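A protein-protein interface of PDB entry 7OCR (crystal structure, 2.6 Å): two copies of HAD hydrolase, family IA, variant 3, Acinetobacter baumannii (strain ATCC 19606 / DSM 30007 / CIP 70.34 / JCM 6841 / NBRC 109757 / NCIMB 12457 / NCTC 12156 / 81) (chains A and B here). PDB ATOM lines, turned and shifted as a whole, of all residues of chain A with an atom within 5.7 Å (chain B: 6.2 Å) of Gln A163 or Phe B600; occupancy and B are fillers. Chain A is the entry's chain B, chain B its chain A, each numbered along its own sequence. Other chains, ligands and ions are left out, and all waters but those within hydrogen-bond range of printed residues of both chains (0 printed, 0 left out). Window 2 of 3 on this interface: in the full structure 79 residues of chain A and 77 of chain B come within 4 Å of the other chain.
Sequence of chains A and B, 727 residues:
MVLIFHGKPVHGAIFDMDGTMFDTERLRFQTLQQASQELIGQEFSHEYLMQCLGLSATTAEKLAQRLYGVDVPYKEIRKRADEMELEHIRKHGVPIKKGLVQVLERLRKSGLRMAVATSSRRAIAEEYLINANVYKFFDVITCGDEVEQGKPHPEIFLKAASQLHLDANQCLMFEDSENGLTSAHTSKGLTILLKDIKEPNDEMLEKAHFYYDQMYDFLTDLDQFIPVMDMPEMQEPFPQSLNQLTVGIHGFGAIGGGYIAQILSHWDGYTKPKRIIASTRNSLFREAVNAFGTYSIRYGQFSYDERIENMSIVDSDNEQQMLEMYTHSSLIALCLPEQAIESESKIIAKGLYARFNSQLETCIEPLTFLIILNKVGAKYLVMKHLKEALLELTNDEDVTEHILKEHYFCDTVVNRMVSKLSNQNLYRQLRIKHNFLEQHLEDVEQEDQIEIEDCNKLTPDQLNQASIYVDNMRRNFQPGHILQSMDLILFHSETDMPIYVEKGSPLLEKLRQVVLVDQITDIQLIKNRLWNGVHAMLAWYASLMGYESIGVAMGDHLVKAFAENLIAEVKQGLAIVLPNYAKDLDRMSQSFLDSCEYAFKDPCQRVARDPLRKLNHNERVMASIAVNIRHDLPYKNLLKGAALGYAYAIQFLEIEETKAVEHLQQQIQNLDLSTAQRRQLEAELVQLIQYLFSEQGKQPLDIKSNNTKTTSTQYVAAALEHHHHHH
Tyr B598 touches Asp A139 (CE2 to OD1, 3.1 Å).
CE1 of Tyr B598 touches O of Gln A163, 3.6 Å away.
Phe B600 touches Gln A163.
CD2 of His A165 touches CE1 of Tyr B598, at 3.6 Å.
Of chain B, only Tyr B598 (3.6 Å) and Phe B600 (3.9 Å) come within 4 Å of Gln A163.
Of the printed residues of chain A, Glu B597 touches His A165.
Of the printed residues of chain B, Leu A164 touches Tyr B598 (2.9 Å).
Thr A142 touches none of the printed residues of chain B.
Val A140 touches none of the printed residues of chain B.
The nearest residue of chain A that does not touch Phe B600 is Asp A139 (4.3 Å).
The nearest printed residue of chain A that does not touch Glu B597 is Leu A164 (4.9 Å).
A ring nitrogen (NE2) of His A165 lies within hydrogen-bond range of the backbone carbonyl oxygen (O) of Gly B551, 2.9 Å away.
A ring nitrogen (NE2) of His A165 is in hydrogen-bond range of the backbone carbonyl oxygen (O) of Glu B597 (2.9 Å).
The side-chain hydroxyl of Tyr B598 sits at hydrogen-bond distance from the backbone carbonyl oxygen of Leu A164.
The backbone carbonyl oxygen (O) of Phe B600 sits at hydrogen-bond distance from the side-chain hydroxyl (OG) of Ser B549, 3.1 Å away.
The backbone NH of Gly B551 is in hydrogen-bond range of the backbone carbonyl oxygen of Ala B599 (3.1 Å).
The side-chain amide nitrogen (NE2) of Gln A163 lies close to the side-chain amino group (NZ) of Lys A159.
The backbone carbonyl oxygen (O) of Ser A162 is in hydrogen-bond range of a ring nitrogen (ND1) of His A165 (3.4 Å).
A ring nitrogen (ND1) of His A165 lies close to the backbone carbonyl oxygen of Gln A163.
No position is printed for both chains.
Of the 7 pairs that touch across the chains among the printed residues, none has its exchanged pair printed and touching as well.
Of the 12 printed residues of chain B, 4 touch a printed residue of chain A.
Hydrophobic or aromatic side chains of chain B within 4 Å of the printed part of chain A: Tyr B598 and Phe B600.
Along chain B the printed residues that touch a printed residue of chain A span positions 551 to 600.
Of the 12 printed residues of chain A, 4 touch a printed residue of chain B.
Printed residues of chain A that touch a printed residue of chain B: Asp A139, Gln A163, Leu A164 and His A165.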
ATOM      1  N   ASP A 139       1.687 -13.876  -4.705  1.00  0.00           N
ATOM      2  CA  ASP A 139       0.998 -12.676  -4.155  1.00  0.00           C
ATOM      3  C   ASP A 139       0.103 -13.100  -2.985  1.00  0.00           C
ATOM      4  O   ASP A 139       0.059 -12.363  -1.979  1.00  0.00           O
ATOM      5  CB  ASP A 139       0.185 -11.959  -5.238  1.00  0.00           C
ATOM      6  CG  ASP A 139       0.988 -11.598  -6.478  1.00  0.00           C
ATOM      7  OD1 ASP A 139       0.955 -10.417  -6.874  1.00  0.00           O
ATOM      8  OD2 ASP A 139       1.634 -12.504  -7.042  1.00  0.00           O
ATOM      9  N   VAL A 140      -0.586 -14.237  -3.126  1.00  0.00           N
ATOM     10  CA  VAL A 140      -1.482 -14.838  -2.091  1.00  0.00           C
ATOM     11  C   VAL A 140      -1.381 -16.366  -2.190  1.00  0.00           C
ATOM     12  O   VAL A 140      -1.021 -16.857  -3.275  1.00  0.00           O
ATOM     13  CB  VAL A 140      -2.937 -14.352  -2.264  1.00  0.00           C
ATOM     14  CG1 VAL A 140      -3.544 -14.818  -3.579  1.00  0.00           C
ATOM     15  CG2 VAL A 140      -3.815 -14.763  -1.091  1.00  0.00           C
ATOM     16  N   ILE A 141      -1.673 -17.081  -1.099  1.00  0.00           N
ATOM     17  CA  ILE A 141      -1.706 -18.575  -1.056  1.00  0.00           C
ATOM     18  C   ILE A 141      -2.997 -19.030  -0.364  1.00  0.00           C
ATOM     19  O   ILE A 141      -3.436 -18.345   0.583  1.00  0.00           O
ATOM     20  CB  ILE A 141      -0.443 -19.147  -0.376  1.00  0.00           C
ATOM     21  CG1 ILE A 141      -0.368 -18.802   1.114  1.00  0.00           C
ATOM     22  CG2 ILE A 141       0.810 -18.701  -1.117  1.00  0.00           C
ATOM     23  CD1 ILE A 141       0.777 -19.472   1.841  1.00  0.00           C
ATOM     24  N   THR A 142      -3.580 -20.136  -0.839  1.00  0.00           N
ATOM     25  CA  THR A 142      -4.786 -20.796  -0.268  1.00  0.00           C
ATOM     26  C   THR A 142      -4.376 -22.165   0.288  1.00  0.00           C
ATOM     27  O   THR A 142      -3.705 -22.918  -0.446  1.00  0.00           O
ATOM     28  CB  THR A 142      -5.901 -20.919  -1.314  1.00  0.00           C
ATOM     29  OG1 THR A 142      -6.052 -19.657  -1.963  1.00  0.00           O
ATOM     30  CG2 THR A 142      -7.226 -21.338  -0.715  1.00  0.00           C
ATOM     31  N   LEU A 158     -10.951 -21.596  -6.775  1.00  0.00           N
ATOM     32  CA  LEU A 158     -11.830 -20.410  -6.978  1.00  0.00           C
ATOM     33  C   LEU A 158     -11.414 -19.293  -6.012  1.00  0.00           C
ATOM     34  O   LEU A 158     -11.363 -18.127  -6.451  1.00  0.00           O
ATOM     35  CB  LEU A 158     -13.293 -20.809  -6.759  1.00  0.00           C
ATOM     36  CG  LEU A 158     -13.933 -21.617  -7.889  1.00  0.00           C
ATOM     37  CD1 LEU A 158     -15.202 -22.306  -7.413  1.00  0.00           C
ATOM     38  CD2 LEU A 158     -14.224 -20.734  -9.095  1.00  0.00           C
ATOM     39  N   LYS A 159     -11.133 -19.646  -4.752  1.00  0.00           N
ATOM     40  CA  LYS A 159     -10.712 -18.706  -3.675  1.00  0.00           C
ATOM     41  C   LYS A 159      -9.335 -18.118  -4.012  1.00  0.00           C
ATOM     42  O   LYS A 159      -9.120 -16.923  -3.724  1.00  0.00           O
ATOM     43  CB  LYS A 159     -10.688 -19.427  -2.322  1.00  0.00           C
ATOM     44  CG  LYS A 159     -10.411 -18.541  -1.115  1.00  0.00           C
ATOM     45  CD  LYS A 159     -10.583 -19.258   0.208  1.00  0.00           C
ATOM     46  CE  LYS A 159     -10.239 -18.396   1.405  1.00  0.00           C
ATOM     47  NZ  LYS A 159      -8.800 -18.042   1.437  1.00  0.00           N
ATOM     48  N   ALA A 160      -8.442 -18.929  -4.591  1.00  0.00           N
ATOM     49  CA  ALA A 160      -7.073 -18.537  -5.008  1.00  0.00           C
ATOM     50  C   ALA A 160      -7.150 -17.501  -6.137  1.00  0.00           C
ATOM     51  O   ALA A 160      -6.418 -16.496  -6.064  1.00  0.00           O
ATOM     52  CB  ALA A 160      -6.292 -19.756  -5.431  1.00  0.00           C
ATOM     53  N   ALA A 161      -8.007 -17.743  -7.134  1.00  0.00           N
ATOM     54  CA  ALA A 161      -8.224 -16.870  -8.312  1.00  0.00           C
ATOM     55  C   ALA A 161      -8.886 -15.555  -7.882  1.00  0.00           C
ATOM     56  O   ALA A 161      -8.505 -14.499  -8.424  1.00  0.00           O
ATOM     57  CB  ALA A 161      -9.058 -17.591  -9.342  1.00  0.00           C
ATOM     58  N   SER A 162      -9.840 -15.624  -6.946  1.00  0.00           N
ATOM     59  CA  SER A 162     -10.628 -14.473  -6.431  1.00  0.00           C
ATOM     60  C   SER A 162      -9.720 -13.503  -5.661  1.00  0.00           C
ATOM     61  O   SER A 162      -9.914 -12.280  -5.804  1.00  0.00           O
ATOM     62  CB  SER A 162     -11.776 -14.944  -5.574  1.00  0.00           C
ATOM     63  OG  SER A 162     -12.631 -13.862  -5.236  1.00  0.00           O
ATOM     64  N   GLN A 163      -8.769 -14.031  -4.882  1.00  0.00           N
ATOM     65  CA  GLN A 163      -7.821 -13.234  -4.053  1.00  0.00           C
ATOM     66  C   GLN A 163      -6.773 -12.559  -4.950  1.00  0.00           C
ATOM     67  O   GLN A 163      -6.183 -11.558  -4.498  1.00  0.00           O
ATOM     68  CB  GLN A 163      -7.160 -14.114  -2.990  1.00  0.00           C
ATOM     69  CG  GLN A 163      -8.061 -14.397  -1.796  1.00  0.00           C
ATOM     70  CD  GLN A 163      -7.391 -15.248  -0.746  1.00  0.00           C
ATOM     71  OE1 GLN A 163      -6.674 -16.200  -1.051  1.00  0.00           O
ATOM     72  NE2 GLN A 163      -7.629 -14.914   0.512  1.00  0.00           N
ATOM     73  N   LEU A 164      -6.549 -13.084  -6.162  1.00  0.00           N
ATOM     74  CA  LEU A 164      -5.648 -12.488  -7.189  1.00  0.00           C
ATOM     75  C   LEU A 164      -6.400 -11.420  -7.997  1.00  0.00           C
ATOM     76  O   LEU A 164      -5.741 -10.717  -8.788  1.00  0.00           O
ATOM     77  CB  LEU A 164      -5.121 -13.593  -8.112  1.00  0.00           C
ATOM     78  CG  LEU A 164      -4.108 -14.554  -7.493  1.00  0.00           C
ATOM     79  CD1 LEU A 164      -3.883 -15.756  -8.400  1.00  0.00           C
ATOM     80  CD2 LEU A 164      -2.793 -13.846  -7.200  1.00  0.00           C
ATOM     81  N   HIS A 165      -7.722 -11.315  -7.808  1.00  0.00           N
ATOM     82  CA  HIS A 165      -8.625 -10.347  -8.491  1.00  0.00           C
ATOM     83  C   HIS A 165      -8.699 -10.691  -9.984  1.00  0.00           C
ATOM     84  O   HIS A 165      -8.608  -9.765 -10.815  1.00  0.00           O
ATOM     85  CB  HIS A 165      -8.173  -8.903  -8.220  1.00  0.00           C
ATOM     86  CG  HIS A 165      -7.766  -8.662  -6.805  1.00  0.00           C
ATOM     87  ND1 HIS A 165      -8.452  -9.211  -5.740  1.00  0.00           N
ATOM     88  CD2 HIS A 165      -6.750  -7.949  -6.276  1.00  0.00           C
ATOM     89  CE1 HIS A 165      -7.877  -8.844  -4.614  1.00  0.00           C
ATOM     90  NE2 HIS A 165      -6.830  -8.068  -4.916  1.00  0.00           N
ATOM     91  N   SER B 549     -10.278  -5.563   4.628  1.00  0.00           N
ATOM     92  CA  SER B 549      -9.046  -4.976   4.035  1.00  0.00           C
ATOM     93  C   SER B 549      -9.351  -4.347   2.670  1.00  0.00           C
ATOM     94  O   SER B 549     -10.324  -4.778   2.019  1.00  0.00           O
ATOM     95  CB  SER B 549      -7.966  -6.020   3.922  1.00  0.00           C
ATOM     96  OG  SER B 549      -6.761  -5.447   3.437  1.00  0.00           O
ATOM     97  N   ILE B 550      -8.534  -3.369   2.261  1.00  0.00           N
ATOM     98  CA  ILE B 550      -8.599  -2.696   0.928  1.00  0.00           C
ATOM     99  C   ILE B 550      -8.207  -3.719  -0.145  1.00  0.00           C
ATOM    100  O   ILE B 550      -8.932  -3.824  -1.150  1.00  0.00           O
ATOM    101  CB  ILE B 550      -7.688  -1.449   0.882  1.00  0.00           C
ATOM    102  CG1 ILE B 550      -8.109  -0.383   1.900  1.00  0.00           C
ATOM    103  CG2 ILE B 550      -7.616  -0.879  -0.528  1.00  0.00           C
ATOM    104  CD1 ILE B 550      -9.365   0.372   1.530  1.00  0.00           C
ATOM    105  N   GLY B 551      -7.097  -4.433   0.076  1.00  0.00           N
ATOM    106  CA  GLY B 551      -6.553  -5.462  -0.833  1.00  0.00           C
ATOM    107  C   GLY B 551      -7.603  -6.481  -1.240  1.00  0.00           C
ATOM    108  O   GLY B 551      -7.678  -6.795  -2.441  1.00  0.00           O
ATOM    109  N   VAL B 552      -8.391  -6.972  -0.277  1.00  0.00           N
ATOM    110  CA  VAL B 552      -9.475  -7.977  -0.498  1.00  0.00           C
ATOM    111  C   VAL B 552     -10.633  -7.306  -1.249  1.00  0.00           C
ATOM    112  O   VAL B 552     -11.215  -7.963  -2.133  1.00  0.00           O
ATOM    113  CB  VAL B 552      -9.945  -8.600   0.832  1.00  0.00           C
ATOM    114  CG1 VAL B 552     -11.138  -9.526   0.639  1.00  0.00           C
ATOM    115  CG2 VAL B 552      -8.807  -9.324   1.540  1.00  0.00           C
ATOM    116  N   CYS B 596      -2.881  -0.312  -3.648  1.00  0.00           N
ATOM    117  CA  CYS B 596      -4.242  -0.733  -3.211  1.00  0.00           C
ATOM    118  C   CYS B 596      -4.519  -2.194  -3.593  1.00  0.00           C
ATOM    119  O   CYS B 596      -5.233  -2.870  -2.826  1.00  0.00           O
ATOM    120  CB  CYS B 596      -5.319   0.149  -3.832  1.00  0.00           C
ATOM    121  SG  CYS B 596      -5.195   1.889  -3.342  1.00  0.00           S
ATOM    122  N   GLU B 597      -3.984  -2.648  -4.732  1.00  0.00           N
ATOM    123  CA  GLU B 597      -4.284  -3.971  -5.348  1.00  0.00           C
ATOM    124  C   GLU B 597      -4.166  -5.076  -4.290  1.00  0.00           C
ATOM    125  O   GLU B 597      -5.166  -5.787  -4.076  1.00  0.00           O
ATOM    126  CB  GLU B 597      -3.355  -4.238  -6.536  1.00  0.00           C
ATOM    127  CG  GLU B 597      -3.887  -5.284  -7.503  1.00  0.00           C
ATOM    128  CD  GLU B 597      -5.147  -4.888  -8.259  1.00  0.00           C
ATOM    129  OE1 GLU B 597      -5.819  -5.792  -8.794  1.00  0.00           O
ATOM    130  OE2 GLU B 597      -5.451  -3.679  -8.316  1.00  0.00           O
ATOM    131  N   TYR B 598      -2.997  -5.202  -3.653  1.00  0.00           N
ATOM    132  CA  TYR B 598      -2.692  -6.232  -2.623  1.00  0.00           C
ATOM    133  C   TYR B 598      -2.277  -5.546  -1.315  1.00  0.00           C
ATOM    134  O   TYR B 598      -1.169  -5.820  -0.809  1.00  0.00           O
ATOM    135  CB  TYR B 598      -1.623  -7.200  -3.139  1.00  0.00           C
ATOM    136  CG  TYR B 598      -2.009  -7.950  -4.389  1.00  0.00           C
ATOM    137  CD1 TYR B 598      -3.149  -8.738  -4.423  1.00  0.00           C
ATOM    138  CD2 TYR B 598      -1.236  -7.881  -5.537  1.00  0.00           C
ATOM    139  CE1 TYR B 598      -3.516  -9.432  -5.565  1.00  0.00           C
ATOM    140  CE2 TYR B 598      -1.587  -8.569  -6.687  1.00  0.00           C
ATOM    141  CZ  TYR B 598      -2.731  -9.348  -6.701  1.00  0.00           C
ATOM    142  OH  TYR B 598      -3.087 -10.030  -7.829  1.00  0.00           O
ATOM    143  N   ALA B 599      -3.153  -4.682  -0.790  1.00  0.00           N
ATOM    144  CA  ALA B 599      -3.010  -3.991   0.514  1.00  0.00           C
ATOM    145  C   ALA B 599      -3.767  -4.786   1.587  1.00  0.00           C
ATOM    146  O   ALA B 599      -4.785  -4.281   2.102  1.00  0.00           O
ATOM    147  CB  ALA B 599      -3.515  -2.572   0.404  1.00  0.00           C
ATOM    148  N   PHE B 600      -3.277  -5.989   1.902  1.00  0.00           N
ATOM    149  CA  PHE B 600      -3.909  -6.961   2.835  1.00  0.00           C
ATOM    150  C   PHE B 600      -3.608  -6.580   4.291  1.00  0.00           C
ATOM    151  O   PHE B 600      -4.502  -6.751   5.143  1.00  0.00           O
ATOM    152  CB  PHE B 600      -3.424  -8.385   2.545  1.00  0.00           C
ATOM    153  CG  PHE B 600      -3.828  -8.929   1.197  1.00  0.00           C
ATOM    154  CD1 PHE B 600      -5.163  -9.150   0.893  1.00  0.00           C
ATOM    155  CD2 PHE B 600      -2.875  -9.232   0.236  1.00  0.00           C
ATOM    156  CE1 PHE B 600      -5.536  -9.653  -0.344  1.00  0.00           C
ATOM    157  CE2 PHE B 600      -3.249  -9.737  -1.000  1.00  0.00           C
ATOM    158  CZ  PHE B 600      -4.578  -9.948  -1.287  1.00  0.00           C
ATOM    159  N   LYS B 601      -2.396  -6.083   4.559  1.00  0.00           N
ATOM    160  CA  LYS B 601      -1.859  -5.847   5.929  1.00  0.00           C
ATOM    161  C   LYS B 601      -2.659  -4.739   6.626  1.00  0.00           C
ATOM    162  O   LYS B 601      -3.298  -5.039   7.655  1.00  0.00           O
ATOM    163  CB  LYS B 601      -0.367  -5.497   5.870  1.00  0.00           C
ATOM    164  CG  LYS B 601       0.539  -6.580   5.293  1.00  0.00           C
ATOM    165  CD  LYS B 601       0.515  -7.883   6.067  1.00  0.00           C
ATOM    166  CE  LYS B 601       1.485  -8.913   5.527  1.00  0.00           C
ATOM    167  NZ  LYS B 601       1.308 -10.228   6.188  1.00  0.00           N
ATOM    168  N   ASP B 602      -2.622  -3.513   6.091  1.00  0.00           N
ATOM    169  CA  ASP B 602      -3.273  -2.317   6.694  1.00  0.00           C
ATOM    170  C   ASP B 602      -4.791  -2.458   6.577  1.00  0.00           C
ATOM    171  O   ASP B 602      -5.310  -2.679   5.484  1.00  0.00           O
ATOM    172  CB  ASP B 602      -2.765  -1.016   6.062  1.00  0.00           C
ATOM    173  CG  ASP B 602      -3.089  -0.861   4.585  1.00  0.00           C
ATOM    174  OD1 ASP B 602      -2.964  -1.860   3.848  1.00  0.00           O
ATOM    175  OD2 ASP B 602      -3.467   0.257   4.184  1.00  0.00           O
ATOM    176  N   PRO B 603      -5.548  -2.349   7.694  1.00  0.00           N
ATOM    177  CA  PRO B 603      -7.008  -2.451   7.651  1.00  0.00           C
ATOM    178  C   PRO B 603      -7.682  -1.162   7.153  1.00  0.00           C
ATOM    179  O   PRO B 603      -6.989  -0.186   6.918  1.00  0.00           O
ATOM    180  CB  PRO B 603      -7.371  -2.739   9.115  1.00  0.00           C
ATOM    181  CG  PRO B 603      -6.298  -2.021   9.905  1.00  0.00           C
ATOM    182  CD  PRO B 603      -5.045  -2.130   9.060  1.00  0.00           C
